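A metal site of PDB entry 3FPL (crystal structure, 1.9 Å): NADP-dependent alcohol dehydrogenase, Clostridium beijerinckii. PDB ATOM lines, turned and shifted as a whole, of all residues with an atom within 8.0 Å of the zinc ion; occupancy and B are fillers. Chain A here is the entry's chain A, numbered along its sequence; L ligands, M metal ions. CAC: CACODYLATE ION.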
ATOM      1  N   SER A  35     -16.590  22.811  31.917  1.00  0.00           N
ATOM      2  CA  SER A  35     -16.445  22.003  30.749  1.00  0.00           C
ATOM      3  C   SER A  35     -15.042  21.456  30.669  1.00  0.00           C
ATOM      4  O   SER A  35     -14.094  22.144  31.074  1.00  0.00           O
ATOM      5  CB  SER A  35     -16.708  22.866  29.507  1.00  0.00           C
ATOM      6  OG  SER A  35     -16.650  22.088  28.330  1.00  0.00           O
ATOM      7  N   PRO A  36     -14.901  20.223  30.164  1.00  0.00           N
ATOM      8  CA  PRO A  36     -13.534  19.758  29.949  1.00  0.00           C
ATOM      9  C   PRO A  36     -13.051  20.136  28.552  1.00  0.00           C
ATOM     10  O   PRO A  36     -13.894  20.397  27.657  1.00  0.00           O
ATOM     11  CB  PRO A  36     -13.653  18.257  30.094  1.00  0.00           C
ATOM     12  CG  PRO A  36     -15.049  17.946  29.591  1.00  0.00           C
ATOM     13  CD  PRO A  36     -15.898  19.181  29.854  1.00  0.00           C
ATOM     14  N   CYS A  37     -11.734  20.112  28.388  1.00  0.00           N
ATOM     15  CA  CYS A  37     -11.062  20.552  27.173  1.00  0.00           C
ATOM     16  C   CYS A  37     -10.076  19.501  26.670  1.00  0.00           C
ATOM     17  O   CYS A  37      -9.408  18.809  27.448  1.00  0.00           O
ATOM     18  CB  CYS A  37     -10.274  21.845  27.470  1.00  0.00           C
ATOM     19  SG  CYS A  37      -9.599  22.696  26.013  1.00  0.00           S
ATOM     20  N   THR A  38     -10.005  19.412  25.348  1.00  0.00           N
ATOM     21  CA  THR A  38      -9.003  18.623  24.639  1.00  0.00           C
ATOM     22  C   THR A  38      -7.583  18.936  25.103  1.00  0.00           C
ATOM     23  O   THR A  38      -6.701  18.081  25.118  1.00  0.00           O
ATOM     24  CB  THR A  38      -9.181  18.892  23.132  1.00  0.00           C
ATOM     25  OG1 THR A  38     -10.430  18.309  22.708  1.00  0.00           O
ATOM     26  CG2 THR A  38      -8.003  18.359  22.292  1.00  0.00           C
ATOM     27  N   SER A  39      -7.334  20.187  25.470  1.00  0.00           N
ATOM     28  CA  SER A  39      -6.013  20.573  26.008  1.00  0.00           C
ATOM     29  C   SER A  39      -5.596  19.732  27.227  1.00  0.00           C
ATOM     30  O   SER A  39      -4.424  19.322  27.353  1.00  0.00           O
ATOM     31  CB  SER A  39      -5.964  22.061  26.332  1.00  0.00           C
ATOM     32  OG  SER A  39      -6.105  22.828  25.134  1.00  0.00           O
ATOM     33  N   ASP A  40      -6.541  19.436  28.115  1.00  0.00           N
ATOM     34  CA  ASP A  40      -6.198  18.604  29.252  1.00  0.00           C
ATOM     35  C   ASP A  40      -5.817  17.191  28.838  1.00  0.00           C
ATOM     36  O   ASP A  40      -5.054  16.545  29.533  1.00  0.00           O
ATOM     37  CB  ASP A  40      -7.291  18.643  30.329  1.00  0.00           C
ATOM     38  CG  ASP A  40      -7.267  19.895  31.152  1.00  0.00           C
ATOM     39  OD1 ASP A  40      -6.342  20.740  30.989  1.00  0.00           O
ATOM     40  OD2 ASP A  40      -8.186  20.024  32.002  1.00  0.00           O
ATOM     41  N   GLY A  58      -8.981  21.204  34.502  1.00  0.00           N
ATOM     42  CA  GLY A  58     -10.050  22.082  34.071  1.00  0.00           C
ATOM     43  C   GLY A  58      -9.712  23.550  34.090  1.00  0.00           C
ATOM     44  O   GLY A  58      -9.046  24.049  35.011  1.00  0.00           O
ATOM     45  N   HIS A  59     -10.158  24.266  33.070  1.00  0.00           N
ATOM     46  CA  HIS A  59      -9.958  25.719  32.982  1.00  0.00           C
ATOM     47  C   HIS A  59     -11.141  26.460  32.335  1.00  0.00           C
ATOM     48  O   HIS A  59     -10.990  27.593  31.824  1.00  0.00           O
ATOM     49  CB  HIS A  59      -8.623  26.061  32.281  1.00  0.00           C
ATOM     50  CG  HIS A  59      -8.410  25.346  30.983  1.00  0.00           C
ATOM     51  ND1 HIS A  59      -7.684  24.177  30.883  1.00  0.00           N
ATOM     52  CD2 HIS A  59      -8.891  25.600  29.737  1.00  0.00           C
ATOM     53  CE1 HIS A  59      -7.709  23.751  29.626  1.00  0.00           C
ATOM     54  NE2 HIS A  59      -8.424  24.602  28.912  1.00  0.00           N
ATOM     55  N   GLU A  60     -12.322  25.845  32.382  1.00  0.00           N
ATOM     56  CA  GLU A  60     -13.537  26.438  31.799  1.00  0.00           C
ATOM     57  C   GLU A  60     -14.662  26.384  32.796  1.00  0.00           C
ATOM     58  O   GLU A  60     -15.239  25.305  33.048  1.00  0.00           O
ATOM     59  CB  GLU A  60     -13.935  25.709  30.532  1.00  0.00           C
ATOM     60  CG  GLU A  60     -13.003  25.926  29.355  1.00  0.00           C
ATOM     61  CD  GLU A  60     -13.122  24.838  28.313  1.00  0.00           C
ATOM     62  OE1 GLU A  60     -13.758  25.012  27.266  1.00  0.00           O
ATOM     63  OE2 GLU A  60     -12.516  23.777  28.542  1.00  0.00           O
ATOM     64  N   CYS A  85     -10.242  31.579  30.928  1.00  0.00           N
ATOM     65  CA  CYS A  85      -9.257  30.506  31.207  1.00  0.00           C
ATOM     66  C   CYS A  85      -7.844  31.064  31.422  1.00  0.00           C
ATOM     67  O   CYS A  85      -7.002  30.442  32.091  1.00  0.00           O
ATOM     68  CB  CYS A  85      -9.241  29.501  30.077  1.00  0.00           C
ATOM     69  SG  CYS A  85      -8.691  30.152  28.457  1.00  0.00           S
ATOM     70  N   TRP A 110      -1.972  31.698  31.214  1.00  0.00           N
ATOM     71  CA  TRP A 110      -2.898  30.579  31.281  1.00  0.00           C
ATOM     72  C   TRP A 110      -2.427  29.668  32.435  1.00  0.00           C
ATOM     73  O   TRP A 110      -1.464  28.936  32.283  1.00  0.00           O
ATOM     74  CB  TRP A 110      -2.966  29.817  29.951  1.00  0.00           C
ATOM     75  CG  TRP A 110      -3.624  28.421  30.090  1.00  0.00           C
ATOM     76  CD1 TRP A 110      -4.716  28.109  30.842  1.00  0.00           C
ATOM     77  CD2 TRP A 110      -3.198  27.194  29.484  1.00  0.00           C
ATOM     78  NE1 TRP A 110      -4.985  26.750  30.755  1.00  0.00           N
ATOM     79  CE2 TRP A 110      -4.070  26.174  29.924  1.00  0.00           C
ATOM     80  CE3 TRP A 110      -2.138  26.852  28.628  1.00  0.00           C
ATOM     81  CZ2 TRP A 110      -3.927  24.835  29.530  1.00  0.00           C
ATOM     82  CZ3 TRP A 110      -2.008  25.520  28.224  1.00  0.00           C
ATOM     83  CH2 TRP A 110      -2.895  24.537  28.667  1.00  0.00           C
ATOM     84  N   PHE A 112      -4.706  27.881  35.082  1.00  0.00           N
ATOM     85  CA  PHE A 112      -5.610  26.772  35.392  1.00  0.00           C
ATOM     86  C   PHE A 112      -5.310  25.560  34.492  1.00  0.00           C
ATOM     87  O   PHE A 112      -5.535  25.622  33.295  1.00  0.00           O
ATOM     88  CB  PHE A 112      -7.093  27.137  35.192  1.00  0.00           C
ATOM     89  CG  PHE A 112      -7.645  28.130  36.174  1.00  0.00           C
ATOM     90  CD1 PHE A 112      -7.438  28.004  37.535  1.00  0.00           C
ATOM     91  CD2 PHE A 112      -8.433  29.200  35.720  1.00  0.00           C
ATOM     92  CE1 PHE A 112      -7.957  28.952  38.444  1.00  0.00           C
ATOM     93  CE2 PHE A 112      -9.004  30.116  36.634  1.00  0.00           C
ATOM     94  CZ  PHE A 112      -8.767  29.969  37.994  1.00  0.00           C
ATOM     95  N   SER A 113      -4.872  24.475  35.105  1.00  0.00           N
ATOM     96  CA  SER A 113      -4.529  23.197  34.441  1.00  0.00           C
ATOM     97  C   SER A 113      -3.431  23.224  33.371  1.00  0.00           C
ATOM     98  O   SER A 113      -3.254  22.265  32.622  1.00  0.00           O
ATOM     99  CB  SER A 113      -5.768  22.441  33.941  1.00  0.00           C
ATOM    100  OG  SER A 113      -6.129  22.729  32.611  1.00  0.00           O
ATOM    101  N   THR A 149     -15.262  31.131  27.983  1.00  0.00           N
ATOM    102  CA  THR A 149     -14.083  31.175  28.806  1.00  0.00           C
ATOM    103  C   THR A 149     -12.868  30.669  28.071  1.00  0.00           C
ATOM    104  O   THR A 149     -11.751  30.995  28.456  1.00  0.00           O
ATOM    105  CB  THR A 149     -14.253  30.358  30.110  1.00  0.00           C
ATOM    106  OG1 THR A 149     -14.442  28.975  29.793  1.00  0.00           O
ATOM    107  CG2 THR A 149     -15.492  30.857  30.935  1.00  0.00           C
ATOM    108  N   ASP A 150     -13.056  29.889  27.026  1.00  0.00           N
ATOM    109  CA  ASP A 150     -11.935  29.290  26.299  1.00  0.00           C
ATOM    110  C   ASP A 150     -12.259  29.143  24.788  1.00  0.00           C
ATOM    111  O   ASP A 150     -11.571  29.665  23.964  1.00  0.00           O
ATOM    112  CB  ASP A 150     -11.570  27.976  26.959  1.00  0.00           C
ATOM    113  CG  ASP A 150     -10.310  27.304  26.369  1.00  0.00           C
ATOM    114  OD1 ASP A 150      -9.644  27.794  25.431  1.00  0.00           O
ATOM    115  OD2 ASP A 150     -10.000  26.208  26.877  1.00  0.00           O
ATOM    116  N   MET A 151     -13.330  28.453  24.450  1.00  0.00           N
ATOM    117  CA  MET A 151     -13.622  28.180  23.038  1.00  0.00           C
ATOM    118  C   MET A 151     -13.817  29.446  22.228  1.00  0.00           C
ATOM    119  O   MET A 151     -13.203  29.598  21.196  1.00  0.00           O
ATOM    120  CB  MET A 151     -14.847  27.249  22.894  1.00  0.00           C
ATOM    121  CG  MET A 151     -14.725  25.886  23.602  1.00  0.00           C
ATOM    122  SD  MET A 151     -13.390  24.900  22.985  1.00  0.00           S
ATOM    123  CE  MET A 151     -12.029  25.385  24.086  1.00  0.00           C
ATOM    124  N   THR A 154     -10.447  31.621  22.223  1.00  0.00           N
ATOM    125  CA  THR A 154      -9.367  31.000  21.442  1.00  0.00           C
ATOM    126  C   THR A 154      -9.683  31.016  19.957  1.00  0.00           C
ATOM    127  O   THR A 154      -8.876  31.510  19.144  1.00  0.00           O
ATOM    128  CB  THR A 154      -9.108  29.587  21.858  1.00  0.00           C
ATOM    129  OG1 THR A 154      -8.820  29.578  23.253  1.00  0.00           O
ATOM    130  CG2 THR A 154      -7.921  28.947  21.049  1.00  0.00           C
ATOM    131  N   VAL A 178     -12.934  24.756  18.865  1.00  0.00           N
ATOM    132  CA  VAL A 178     -12.081  25.924  18.629  1.00  0.00           C
ATOM    133  C   VAL A 178     -12.179  26.384  17.182  1.00  0.00           C
ATOM    134  O   VAL A 178     -12.371  27.605  16.921  1.00  0.00           O
ATOM    135  CB  VAL A 178     -10.616  25.674  19.050  1.00  0.00           C
ATOM    136  CG1 VAL A 178      -9.686  26.763  18.458  1.00  0.00           C
ATOM    137  CG2 VAL A 178     -10.531  25.656  20.609  1.00  0.00           C
ATOM    138  N   TYR A 267      -3.133  23.699  20.099  1.00  0.00           N
ATOM    139  CA  TYR A 267      -2.166  23.272  21.112  1.00  0.00           C
ATOM    140  C   TYR A 267      -1.626  21.932  20.609  1.00  0.00           C
ATOM    141  O   TYR A 267      -2.353  20.921  20.602  1.00  0.00           O
ATOM    142  CB  TYR A 267      -2.883  23.214  22.472  1.00  0.00           C
ATOM    143  CG  TYR A 267      -2.178  22.529  23.624  1.00  0.00           C
ATOM    144  CD1 TYR A 267      -0.810  22.170  23.570  1.00  0.00           C
ATOM    145  CD2 TYR A 267      -2.888  22.218  24.799  1.00  0.00           C
ATOM    146  CE1 TYR A 267      -0.210  21.511  24.681  1.00  0.00           C
ATOM    147  CE2 TYR A 267      -2.287  21.562  25.870  1.00  0.00           C
ATOM    148  CZ  TYR A 267      -0.965  21.185  25.813  1.00  0.00           C
ATOM    149  OH  TYR A 267      -0.398  20.500  26.931  1.00  0.00           O
ATOM    150  N   LEU A 294      -1.586  31.729  22.294  1.00  0.00           N
ATOM    151  CA  LEU A 294      -2.488  31.473  23.429  1.00  0.00           C
ATOM    152  C   LEU A 294      -3.608  32.528  23.486  1.00  0.00           C
ATOM    153  O   LEU A 294      -3.346  33.714  23.275  1.00  0.00           O
ATOM    154  CB  LEU A 294      -1.648  31.557  24.718  1.00  0.00           C
ATOM    155  CG  LEU A 294      -2.334  31.263  26.067  1.00  0.00           C
ATOM    156  CD1 LEU A 294      -3.020  29.898  25.957  1.00  0.00           C
ATOM    157  CD2 LEU A 294      -1.337  31.303  27.216  1.00  0.00           C
ATOM    158  N   CYS A 295      -4.830  32.099  23.831  1.00  0.00           N
ATOM    159  CA  CYS A 295      -5.981  33.024  23.865  1.00  0.00           C
ATOM    160  C   CYS A 295      -5.808  34.078  24.935  1.00  0.00           C
ATOM    161  O   CYS A 295      -5.378  33.760  26.053  1.00  0.00           O
ATOM    162  CB  CYS A 295      -7.272  32.288  24.169  1.00  0.00           C
ATOM    163  SG  CYS A 295      -7.315  31.475  25.799  1.00  0.00           S
ATOM    164  N   LYS A 346     -18.879  20.117  22.720  1.00  0.00           N
ATOM    165  CA  LYS A 346     -18.528  20.350  24.119  1.00  0.00           C
ATOM    166  C   LYS A 346     -19.557  19.762  25.108  1.00  0.00           C
ATOM    167  O   LYS A 346     -20.754  19.698  24.826  1.00  0.00           O
ATOM    168  CB  LYS A 346     -18.338  21.844  24.408  1.00  0.00           C
ATOM    169  CG  LYS A 346     -17.121  22.489  23.661  1.00  0.00           C
ATOM    170  CD  LYS A 346     -15.747  22.148  24.212  1.00  0.00           C
ATOM    171  CE  LYS A 346     -15.404  22.910  25.460  1.00  0.00           C
ATOM    172  NZ  LYS A 346     -14.029  22.648  25.847  1.00  0.00           N
HETATM  173 AS   CAC L   1      -6.348  26.482  25.856  1.00  0.00          AS
HETATM  174  O1  CAC L   1      -7.010  24.895  26.067  1.00  0.00           O
HETATM  175  O2  CAC L   1      -7.235  27.196  24.511  1.00  0.00           O
HETATM  176  C1  CAC L   1      -6.378  27.697  27.377  1.00  0.00           C
HETATM  177  C2  CAC L   1      -4.546  26.204  25.129  1.00  0.00           C
HETATM  178 ZN    ZN M   1      -8.856  24.593  26.899  1.00  0.00          ZN
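The zinc ion is bound by OD2 of Asp 150 (2.0 Å), O1 of the ligand (2.0 Å), NE2 of His 59 (2.1 Å) and SG of Cys 37 (2.2 Å).
The side-chain hydroxyl (OG1) of Thr 154 lies within hydrogen-bond range of the backbone carbonyl oxygen (O) of Asp 150, at 2.8 Å.
A ring nitrogen (ND1) of His 59 sits at hydrogen-bond distance from the side-chain hydroxyl (OG) of Ser 113 (2.7 Å).
The side-chain sulfur (SG) of Cys 37 sits close to the backbone NH (N) of Ser 39, 3.4 Å away.
Residues that only touch the zinc ion: Ser 39.
Within 4 Å of the zinc ion: Cys 37, Ser 39, His 59 and Asp 150.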
